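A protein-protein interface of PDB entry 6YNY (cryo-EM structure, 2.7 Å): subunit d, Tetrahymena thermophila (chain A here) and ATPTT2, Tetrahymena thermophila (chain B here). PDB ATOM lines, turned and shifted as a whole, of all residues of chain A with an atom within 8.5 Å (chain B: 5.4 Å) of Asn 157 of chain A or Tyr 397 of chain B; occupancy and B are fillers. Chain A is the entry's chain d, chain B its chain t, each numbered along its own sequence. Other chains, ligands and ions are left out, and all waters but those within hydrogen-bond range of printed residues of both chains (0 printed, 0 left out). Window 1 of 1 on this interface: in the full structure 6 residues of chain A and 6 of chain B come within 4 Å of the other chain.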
ATOM      1  N   GLU A 152      -0.337 -10.527  24.821  1.00  0.00           N
ATOM      2  CA  GLU A 152      -1.085 -10.625  23.575  1.00  0.00           C
ATOM      3  C   GLU A 152      -0.202 -11.101  22.433  1.00  0.00           C
ATOM      4  O   GLU A 152      -0.697 -11.703  21.474  1.00  0.00           O
ATOM      5  CB  GLU A 152      -1.693  -9.270  23.225  1.00  0.00           C
ATOM      6  CG  GLU A 152      -2.685  -8.732  24.236  1.00  0.00           C
ATOM      7  CD  GLU A 152      -4.001  -9.483  24.232  1.00  0.00           C
ATOM      8  OE1 GLU A 152      -4.184 -10.367  23.370  1.00  0.00           O
ATOM      9  OE2 GLU A 152      -4.857  -9.184  25.091  1.00  0.00           O
ATOM     10  N   LEU A 153       1.101 -10.842  22.517  1.00  0.00           N
ATOM     11  CA  LEU A 153       2.011 -11.199  21.440  1.00  0.00           C
ATOM     12  C   LEU A 153       2.176 -12.704  21.294  1.00  0.00           C
ATOM     13  O   LEU A 153       2.671 -13.162  20.259  1.00  0.00           O
ATOM     14  CB  LEU A 153       3.368 -10.548  21.684  1.00  0.00           C
ATOM     15  CG  LEU A 153       4.346 -10.572  20.518  1.00  0.00           C
ATOM     16  CD1 LEU A 153       3.896  -9.615  19.437  1.00  0.00           C
ATOM     17  CD2 LEU A 153       5.732 -10.235  20.999  1.00  0.00           C
ATOM     18  N   GLU A 154       1.782 -13.481  22.301  1.00  0.00           N
ATOM     19  CA  GLU A 154       1.907 -14.930  22.208  1.00  0.00           C
ATOM     20  C   GLU A 154       0.987 -15.509  21.145  1.00  0.00           C
ATOM     21  O   GLU A 154       1.280 -16.573  20.589  1.00  0.00           O
ATOM     22  CB  GLU A 154       1.615 -15.566  23.562  1.00  0.00           C
ATOM     23  CG  GLU A 154       2.543 -15.108  24.663  1.00  0.00           C
ATOM     24  CD  GLU A 154       2.152 -15.655  26.019  1.00  0.00           C
ATOM     25  OE1 GLU A 154       1.255 -16.523  26.079  1.00  0.00           O
ATOM     26  OE2 GLU A 154       2.737 -15.213  27.029  1.00  0.00           O
ATOM     27  N   GLU A 155      -0.125 -14.836  20.852  1.00  0.00           N
ATOM     28  CA  GLU A 155      -1.034 -15.292  19.810  1.00  0.00           C
ATOM     29  C   GLU A 155      -0.607 -14.854  18.420  1.00  0.00           C
ATOM     30  O   GLU A 155      -1.220 -15.285  17.437  1.00  0.00           O
ATOM     31  CB  GLU A 155      -2.448 -14.780  20.080  1.00  0.00           C
ATOM     32  CG  GLU A 155      -2.991 -15.108  21.455  1.00  0.00           C
ATOM     33  CD  GLU A 155      -4.452 -14.741  21.594  1.00  0.00           C
ATOM     34  OE1 GLU A 155      -5.110 -14.518  20.557  1.00  0.00           O
ATOM     35  OE2 GLU A 155      -4.947 -14.675  22.737  1.00  0.00           O
ATOM     36  N   TYR A 156       0.409 -14.009  18.311  1.00  0.00           N
ATOM     37  CA  TYR A 156       0.899 -13.516  17.035  1.00  0.00           C
ATOM     38  C   TYR A 156       2.135 -14.315  16.647  1.00  0.00           C
ATOM     39  O   TYR A 156       3.122 -14.333  17.388  1.00  0.00           O
ATOM     40  CB  TYR A 156       1.221 -12.028  17.136  1.00  0.00           C
ATOM     41  CG  TYR A 156       1.466 -11.339  15.821  1.00  0.00           C
ATOM     42  CD1 TYR A 156       0.489 -11.298  14.845  1.00  0.00           C
ATOM     43  CD2 TYR A 156       2.667 -10.707  15.566  1.00  0.00           C
ATOM     44  CE1 TYR A 156       0.707 -10.663  13.650  1.00  0.00           C
ATOM     45  CE2 TYR A 156       2.894 -10.068  14.375  1.00  0.00           C
ATOM     46  CZ  TYR A 156       1.913 -10.049  13.420  1.00  0.00           C
ATOM     47  OH  TYR A 156       2.141  -9.408  12.229  1.00  0.00           O
ATOM     48  N   ASN A 157       2.078 -14.978  15.495  1.00  0.00           N
ATOM     49  CA  ASN A 157       3.182 -15.807  15.040  1.00  0.00           C
ATOM     50  C   ASN A 157       3.239 -15.797  13.522  1.00  0.00           C
ATOM     51  O   ASN A 157       2.209 -15.904  12.853  1.00  0.00           O
ATOM     52  CB  ASN A 157       3.052 -17.238  15.567  1.00  0.00           C
ATOM     53  CG  ASN A 157       1.902 -17.981  14.947  1.00  0.00           C
ATOM     54  OD1 ASN A 157       1.944 -18.348  13.773  1.00  0.00           O
ATOM     55  ND2 ASN A 157       0.870 -18.232  15.741  1.00  0.00           N
ATOM     56  N   ASP A 158       4.452 -15.695  12.990  1.00  0.00           N
ATOM     57  CA  ASP A 158       4.701 -15.660  11.555  1.00  0.00           C
ATOM     58  C   ASP A 158       3.950 -14.503  10.915  1.00  0.00           C
ATOM     59  O   ASP A 158       2.940 -14.713  10.233  1.00  0.00           O
ATOM     60  CB  ASP A 158       4.310 -16.978  10.888  1.00  0.00           C
ATOM     61  CG  ASP A 158       5.290 -18.090  11.178  1.00  0.00           C
ATOM     62  OD1 ASP A 158       6.143 -17.912  12.072  1.00  0.00           O
ATOM     63  OD2 ASP A 158       5.216 -19.138  10.503  1.00  0.00           O
ATOM     64  N   PRO A 159       4.405 -13.270  11.122  1.00  0.00           N
ATOM     65  CA  PRO A 159       3.750 -12.126  10.474  1.00  0.00           C
ATOM     66  C   PRO A 159       3.653 -12.268   8.971  1.00  0.00           C
ATOM     67  O   PRO A 159       2.766 -11.672   8.348  1.00  0.00           O
ATOM     68  CB  PRO A 159       4.645 -10.947  10.875  1.00  0.00           C
ATOM     69  CG  PRO A 159       5.343 -11.402  12.098  1.00  0.00           C
ATOM     70  CD  PRO A 159       5.552 -12.856  11.943  1.00  0.00           C
ATOM     71  N   ASN A 160       4.549 -13.042   8.366  1.00  0.00           N
ATOM     72  CA  ASN A 160       4.568 -13.235   6.926  1.00  0.00           C
ATOM     73  C   ASN A 160       3.570 -14.279   6.450  1.00  0.00           C
ATOM     74  O   ASN A 160       3.408 -14.447   5.238  1.00  0.00           O
ATOM     75  CB  ASN A 160       5.976 -13.626   6.479  1.00  0.00           C
ATOM     76  CG  ASN A 160       6.950 -12.470   6.548  1.00  0.00           C
ATOM     77  OD1 ASN A 160       6.656 -11.367   6.090  1.00  0.00           O
ATOM     78  ND2 ASN A 160       8.113 -12.713   7.131  1.00  0.00           N
ATOM     79  N   ASP A 161       2.903 -14.983   7.364  1.00  0.00           N
ATOM     80  CA  ASP A 161       1.920 -15.995   7.007  1.00  0.00           C
ATOM     81  C   ASP A 161       0.499 -15.591   7.376  1.00  0.00           C
ATOM     82  O   ASP A 161      -0.392 -16.445   7.394  1.00  0.00           O
ATOM     83  CB  ASP A 161       2.275 -17.326   7.669  1.00  0.00           C
ATOM     84  CG  ASP A 161       3.492 -17.979   7.046  1.00  0.00           C
ATOM     85  OD1 ASP A 161       4.015 -17.439   6.049  1.00  0.00           O
ATOM     86  OD2 ASP A 161       3.924 -19.037   7.551  1.00  0.00           O
ATOM     87  N   TYR A 162       0.267 -14.321   7.677  1.00  0.00           N
ATOM     88  CA  TYR A 162      -1.069 -13.811   7.928  1.00  0.00           C
ATOM     89  C   TYR A 162      -1.585 -13.079   6.699  1.00  0.00           C
ATOM     90  O   TYR A 162      -0.817 -12.513   5.919  1.00  0.00           O
ATOM     91  CB  TYR A 162      -1.096 -12.858   9.122  1.00  0.00           C
ATOM     92  CG  TYR A 162      -0.914 -13.512  10.464  1.00  0.00           C
ATOM     93  CD1 TYR A 162       0.208 -13.262  11.229  1.00  0.00           C
ATOM     94  CD2 TYR A 162      -1.872 -14.369  10.973  1.00  0.00           C
ATOM     95  CE1 TYR A 162       0.372 -13.847  12.456  1.00  0.00           C
ATOM     96  CE2 TYR A 162      -1.712 -14.959  12.198  1.00  0.00           C
ATOM     97  CZ  TYR A 162      -0.591 -14.697  12.936  1.00  0.00           C
ATOM     98  OH  TYR A 162      -0.437 -15.292  14.163  1.00  0.00           O
ATOM     99  N   GLU A 166      -5.994  -9.609   8.271  1.00  0.00           N
ATOM    100  CA  GLU A 166      -5.866 -10.206   9.594  1.00  0.00           C
ATOM    101  C   GLU A 166      -4.739  -9.554  10.383  1.00  0.00           C
ATOM    102  O   GLU A 166      -4.844  -9.391  11.602  1.00  0.00           O
ATOM    103  CB  GLU A 166      -5.633 -11.709   9.474  1.00  0.00           C
ATOM    104  CG  GLU A 166      -5.565 -12.435  10.804  1.00  0.00           C
ATOM    105  CD  GLU A 166      -5.519 -13.939  10.651  1.00  0.00           C
ATOM    106  OE1 GLU A 166      -5.292 -14.417   9.520  1.00  0.00           O
ATOM    107  OE2 GLU A 166      -5.714 -14.645  11.661  1.00  0.00           O
ATOM    108  N   ASN A 167      -3.654  -9.182   9.705  1.00  0.00           N
ATOM    109  CA  ASN A 167      -2.575  -8.468  10.374  1.00  0.00           C
ATOM    110  C   ASN A 167      -3.034  -7.097  10.851  1.00  0.00           C
ATOM    111  O   ASN A 167      -2.692  -6.672  11.960  1.00  0.00           O
ATOM    112  CB  ASN A 167      -1.381  -8.331   9.437  1.00  0.00           C
ATOM    113  CG  ASN A 167      -0.227  -9.214   9.829  1.00  0.00           C
ATOM    114  OD1 ASN A 167      -0.020  -9.505  11.004  1.00  0.00           O
ATOM    115  ND2 ASN A 167       0.543  -9.637   8.847  1.00  0.00           N
ATOM    116  N   PHE A 170      -4.859  -7.431  14.163  1.00  0.00           N
ATOM    117  CA  PHE A 170      -3.978  -7.498  15.323  1.00  0.00           C
ATOM    118  C   PHE A 170      -3.539  -6.104  15.742  1.00  0.00           C
ATOM    119  O   PHE A 170      -3.608  -5.743  16.922  1.00  0.00           O
ATOM    120  CB  PHE A 170      -2.757  -8.359  15.014  1.00  0.00           C
ATOM    121  CG  PHE A 170      -2.981  -9.826  15.178  1.00  0.00           C
ATOM    122  CD1 PHE A 170      -3.195 -10.372  16.427  1.00  0.00           C
ATOM    123  CD2 PHE A 170      -2.950 -10.669  14.086  1.00  0.00           C
ATOM    124  CE1 PHE A 170      -3.390 -11.719  16.578  1.00  0.00           C
ATOM    125  CE2 PHE A 170      -3.143 -12.014  14.235  1.00  0.00           C
ATOM    126  CZ  PHE A 170      -3.363 -12.542  15.482  1.00  0.00           C
ATOM    127  N   ARG B 327       7.264 -31.725  12.463  1.00  0.00           N
ATOM    128  CA  ARG B 327       7.687 -30.338  12.588  1.00  0.00           C
ATOM    129  C   ARG B 327       9.187 -30.248  12.828  1.00  0.00           C
ATOM    130  O   ARG B 327       9.745 -30.972  13.654  1.00  0.00           O
ATOM    131  CB  ARG B 327       6.942 -29.669  13.736  1.00  0.00           C
ATOM    132  CG  ARG B 327       5.441 -29.607  13.560  1.00  0.00           C
ATOM    133  CD  ARG B 327       5.025 -28.427  12.719  1.00  0.00           C
ATOM    134  NE  ARG B 327       3.580 -28.351  12.558  1.00  0.00           N
ATOM    135  CZ  ARG B 327       2.939 -27.304  12.057  1.00  0.00           C
ATOM    136  NH1 ARG B 327       3.612 -26.232  11.671  1.00  0.00           N
ATOM    137  NH2 ARG B 327       1.623 -27.327  11.945  1.00  0.00           N
ATOM    138  N   HIS B 329      12.423 -27.181  13.030  1.00  0.00           N
ATOM    139  CA  HIS B 329      12.894 -25.806  13.019  1.00  0.00           C
ATOM    140  C   HIS B 329      14.408 -25.807  13.127  1.00  0.00           C
ATOM    141  O   HIS B 329      14.975 -26.520  13.959  1.00  0.00           O
ATOM    142  CB  HIS B 329      12.275 -25.000  14.158  1.00  0.00           C
ATOM    143  CG  HIS B 329      10.918 -24.457  13.844  1.00  0.00           C
ATOM    144  ND1 HIS B 329       9.956 -25.192  13.186  1.00  0.00           N
ATOM    145  CD2 HIS B 329      10.360 -23.251  14.102  1.00  0.00           C
ATOM    146  CE1 HIS B 329       8.865 -24.461  13.050  1.00  0.00           C
ATOM    147  NE2 HIS B 329       9.084 -23.280  13.598  1.00  0.00           N
ATOM    148  N   LYS B 392       9.011 -20.260  20.928  1.00  0.00           N
ATOM    149  CA  LYS B 392       7.957 -20.124  19.932  1.00  0.00           C
ATOM    150  C   LYS B 392       7.642 -21.468  19.290  1.00  0.00           C
ATOM    151  O   LYS B 392       6.476 -21.784  19.033  1.00  0.00           O
ATOM    152  CB  LYS B 392       8.371 -19.102  18.877  1.00  0.00           C
ATOM    153  CG  LYS B 392       7.228 -18.558  18.055  1.00  0.00           C
ATOM    154  CD  LYS B 392       6.328 -17.671  18.889  1.00  0.00           C
ATOM    155  CE  LYS B 392       5.186 -17.122  18.082  1.00  0.00           C
ATOM    156  NZ  LYS B 392       4.304 -16.254  18.904  1.00  0.00           N
ATOM    157  N   PHE B 393       8.674 -22.270  19.029  1.00  0.00           N
ATOM    158  CA  PHE B 393       8.467 -23.594  18.458  1.00  0.00           C
ATOM    159  C   PHE B 393       7.733 -24.504  19.431  1.00  0.00           C
ATOM    160  O   PHE B 393       6.833 -25.251  19.033  1.00  0.00           O
ATOM    161  CB  PHE B 393       9.810 -24.197  18.066  1.00  0.00           C
ATOM    162  CG  PHE B 393       9.725 -25.611  17.596  1.00  0.00           C
ATOM    163  CD1 PHE B 393       9.239 -25.906  16.341  1.00  0.00           C
ATOM    164  CD2 PHE B 393      10.143 -26.645  18.404  1.00  0.00           C
ATOM    165  CE1 PHE B 393       9.163 -27.203  15.906  1.00  0.00           C
ATOM    166  CE2 PHE B 393      10.068 -27.943  17.973  1.00  0.00           C
ATOM    167  CZ  PHE B 393       9.578 -28.223  16.721  1.00  0.00           C
ATOM    168  N   LEU B 394       8.103 -24.456  20.710  1.00  0.00           N
ATOM    169  CA  LEU B 394       7.461 -25.308  21.701  1.00  0.00           C
ATOM    170  C   LEU B 394       6.031 -24.868  21.972  1.00  0.00           C
ATOM    171  O   LEU B 394       5.167 -25.708  22.246  1.00  0.00           O
ATOM    172  CB  LEU B 394       8.268 -25.292  22.996  1.00  0.00           C
ATOM    173  CG  LEU B 394       9.715 -25.767  22.895  1.00  0.00           C
ATOM    174  CD1 LEU B 394      10.455 -25.553  24.196  1.00  0.00           C
ATOM    175  CD2 LEU B 394       9.764 -27.215  22.500  1.00  0.00           C
ATOM    176  N   HIS B 395       5.763 -23.567  21.898  1.00  0.00           N
ATOM    177  CA  HIS B 395       4.463 -23.050  22.297  1.00  0.00           C
ATOM    178  C   HIS B 395       3.430 -23.176  21.182  1.00  0.00           C
ATOM    179  O   HIS B 395       2.277 -23.533  21.444  1.00  0.00           O
ATOM    180  CB  HIS B 395       4.594 -21.591  22.728  1.00  0.00           C
ATOM    181  CG  HIS B 395       3.323 -21.003  23.249  1.00  0.00           C
ATOM    182  ND1 HIS B 395       2.799 -21.335  24.479  1.00  0.00           N
ATOM    183  CD2 HIS B 395       2.467 -20.106  22.706  1.00  0.00           C
ATOM    184  CE1 HIS B 395       1.679 -20.664  24.673  1.00  0.00           C
ATOM    185  NE2 HIS B 395       1.454 -19.913  23.612  1.00  0.00           N
ATOM    186  N   SER B 396       3.814 -22.881  19.943  1.00  0.00           N
ATOM    187  CA  SER B 396       2.858 -22.753  18.855  1.00  0.00           C
ATOM    188  C   SER B 396       3.000 -23.788  17.748  1.00  0.00           C
ATOM    189  O   SER B 396       2.002 -24.097  17.096  1.00  0.00           O
ATOM    190  CB  SER B 396       2.963 -21.356  18.231  1.00  0.00           C
ATOM    191  OG  SER B 396       4.295 -21.060  17.866  1.00  0.00           O
ATOM    192  N   TYR B 397       4.191 -24.337  17.516  1.00  0.00           N
ATOM    193  CA  TYR B 397       4.431 -25.183  16.355  1.00  0.00           C
ATOM    194  C   TYR B 397       4.704 -26.641  16.677  1.00  0.00           C
ATOM    195  O   TYR B 397       4.341 -27.508  15.882  1.00  0.00           O
ATOM    196  CB  TYR B 397       5.604 -24.644  15.533  1.00  0.00           C
ATOM    197  CG  TYR B 397       5.402 -23.237  15.050  1.00  0.00           C
ATOM    198  CD1 TYR B 397       4.550 -22.965  13.994  1.00  0.00           C
ATOM    199  CD2 TYR B 397       6.065 -22.180  15.643  1.00  0.00           C
ATOM    200  CE1 TYR B 397       4.363 -21.684  13.549  1.00  0.00           C
ATOM    201  CE2 TYR B 397       5.883 -20.895  15.206  1.00  0.00           C
ATOM    202  CZ  TYR B 397       5.032 -20.650  14.157  1.00  0.00           C
ATOM    203  OH  TYR B 397       4.845 -19.366  13.716  1.00  0.00           O
ATOM    204  N   ASP B 398       5.326 -26.941  17.809  1.00  0.00           N
ATOM    205  CA  ASP B 398       5.677 -28.321  18.105  1.00  0.00           C
ATOM    206  C   ASP B 398       4.438 -29.117  18.488  1.00  0.00           C
ATOM    207  O   ASP B 398       3.580 -28.649  19.239  1.00  0.00           O
ATOM    208  CB  ASP B 398       6.705 -28.381  19.229  1.00  0.00           C
ATOM    209  CG  ASP B 398       7.128 -29.791  19.552  1.00  0.00           C
ATOM    210  OD1 ASP B 398       6.840 -30.700  18.750  1.00  0.00           O
ATOM    211  OD2 ASP B 398       7.734 -29.993  20.622  1.00  0.00           O
ATOM    212  N   GLY B 399       4.359 -30.337  17.963  1.00  0.00           N
ATOM    213  CA  GLY B 399       3.236 -31.208  18.237  1.00  0.00           C
ATOM    214  C   GLY B 399       1.934 -30.711  17.661  1.00  0.00           C
ATOM    215  O   GLY B 399       0.871 -30.971  18.229  1.00  0.00           O
ATOM    216  N   VAL B 400       1.992 -30.006  16.539  1.00  0.00           N
ATOM    217  CA  VAL B 400       0.816 -29.512  15.839  1.00  0.00           C
ATOM    218  C   VAL B 400       0.716 -30.238  14.509  1.00  0.00           C
ATOM    219  O   VAL B 400       1.727 -30.474  13.838  1.00  0.00           O
ATOM    220  CB  VAL B 400       0.878 -27.988  15.632  1.00  0.00           C
ATOM    221  CG1 VAL B 400      -0.305 -27.520  14.832  1.00  0.00           C
ATOM    222  CG2 VAL B 400       0.907 -27.283  16.956  1.00  0.00           C
ATOM    223  N   LYS B 405      -1.723 -24.449  10.690  1.00  0.00           N
ATOM    224  CA  LYS B 405      -0.675 -23.440  10.773  1.00  0.00           C
ATOM    225  C   LYS B 405      -0.016 -23.452  12.144  1.00  0.00           C
ATOM    226  O   LYS B 405       1.196 -23.657  12.267  1.00  0.00           O
ATOM    227  CB  LYS B 405      -1.253 -22.056  10.484  1.00  0.00           C
ATOM    228  CG  LYS B 405      -1.509 -21.765   9.028  1.00  0.00           C
ATOM    229  CD  LYS B 405      -0.241 -21.733   8.197  1.00  0.00           C
ATOM    230  CE  LYS B 405       0.730 -20.699   8.686  1.00  0.00           C
ATOM    231  NZ  LYS B 405       1.875 -20.573   7.758  1.00  0.00           N
ATOM    232  N   ASP B 406      -0.807 -23.234  13.188  1.00  0.00           N
ATOM    233  CA  ASP B 406      -0.297 -23.048  14.534  1.00  0.00           C
ATOM    234  C   ASP B 406      -1.189 -23.800  15.505  1.00  0.00           C
ATOM    235  O   ASP B 406      -2.163 -24.450  15.116  1.00  0.00           O
ATOM    236  CB  ASP B 406      -0.246 -21.563  14.902  1.00  0.00           C
ATOM    237  CG  ASP B 406       0.401 -20.723  13.837  1.00  0.00           C
ATOM    238  OD1 ASP B 406       1.470 -21.124  13.333  1.00  0.00           O
ATOM    239  OD2 ASP B 406      -0.171 -19.669  13.491  1.00  0.00           O
ATOM    240  N   ARG B 407      -0.844 -23.705  16.786  1.00  0.00           N
ATOM    241  CA  ARG B 407      -1.676 -24.285  17.826  1.00  0.00           C
ATOM    242  C   ARG B 407      -2.993 -23.538  17.963  1.00  0.00           C
ATOM    243  O   ARG B 407      -3.964 -24.098  18.480  1.00  0.00           O
ATOM    244  CB  ARG B 407      -0.916 -24.282  19.147  1.00  0.00           C
ATOM    245  CG  ARG B 407      -1.318 -25.382  20.079  1.00  0.00           C
ATOM    246  CD  ARG B 407      -0.351 -25.515  21.228  1.00  0.00           C
ATOM    247  NE  ARG B 407      -0.503 -26.794  21.905  1.00  0.00           N
ATOM    248  CZ  ARG B 407       0.099 -27.912  21.522  1.00  0.00           C
ATOM    249  NH1 ARG B 407       0.896 -27.920  20.470  1.00  0.00           N
ATOM    250  NH2 ARG B 407      -0.097 -29.026  22.196  1.00  0.00           N
ATOM    251  N   THR B 408      -3.036 -22.284  17.513  1.00  0.00           N
ATOM    252  CA  THR B 408      -4.266 -21.503  17.554  1.00  0.00           C
ATOM    253  C   THR B 408      -5.377 -22.152  16.739  1.00  0.00           C
ATOM    254  O   THR B 408      -6.557 -21.984  17.059  1.00  0.00           O
ATOM    255  CB  THR B 408      -3.998 -20.093  17.034  1.00  0.00           C
ATOM    256  OG1 THR B 408      -3.323 -20.173  15.772  1.00  0.00           O
ATOM    257  CG2 THR B 408      -3.149 -19.312  18.009  1.00  0.00           C
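The backbone carbonyl oxygen (O) of Lys 392 of chain B is in hydrogen-bond range of the side-chain hydroxyl (OG) of Ser 396 of chain B, 2.6 Å away.
The side-chain hydroxyl (OH) of Tyr 156 of chain A is in hydrogen-bond range of the side-chain amide oxygen (OD1) of Asn 167 of chain A (2.5 Å).
The backbone NH (N) of Asn 157 of chain A is in hydrogen-bond range of the side-chain hydroxyl (OH) of Tyr 162 of chain A, at 2.9 Å.
Hydrophobic or aromatic side chains of chain B that line the printed part of chain A: Tyr 397.
Of the 14 printed residues of chain A, 6 touch a printed residue of chain B.
NZ of Lys 392 of chain B sits at hydrogen-bond distance from O of Glu 154 of chain A (3.5 Å).
The backbone carbonyl oxygen of Tyr 156 of chain A is in hydrogen-bond range of the side-chain amino group of Lys 392 of chain B.
The side-chain amide oxygen of Asn 157 of chain A lies within hydrogen-bond range of the side-chain hydroxyl of Tyr 397 of chain B (3.1 Å).
The side-chain hydroxyl of Tyr 397 of chain B is in hydrogen-bond range of the side-chain carboxylate of Asp 158 of chain A (2.5 Å).
OD2 of Asp 161 of chain A lies within salt-bridge range of NZ of Lys 405 of chain B (2.6 Å).
The side-chain amide oxygen (OD1) of Asn 157 of chain A sits close to the side-chain carboxylate (OD2) of Asp 406 of chain B (2.5 Å).
Among the printed residues, merely in contact across the chains: Asn 157 of chain A with Lys 392 of chain B and Leu 153 of chain A with Lys 392 of chain B.
Of the printed residues of chain B, Glu 154 of chain A touches Lys 392 (3.5 Å).
Printed residues of chain B within 4 Å of Asp 161 of chain A: Lys 405.
Of the printed residues of chain A, Lys 392 of chain B touches Leu 153, Glu 154, Tyr 156 and Asn 157.
No residue of chain A comes within 4 Å of Ser 396 of chain B.
Of chain A, only Asn 157 (3.1 Å) and Asp 158 (2.5 Å) come within 4 Å of Tyr 397 of chain B.
The nearest residue of chain B that does not touch Asn 157 of chain A is Ser 396 of chain B (4.5 Å).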
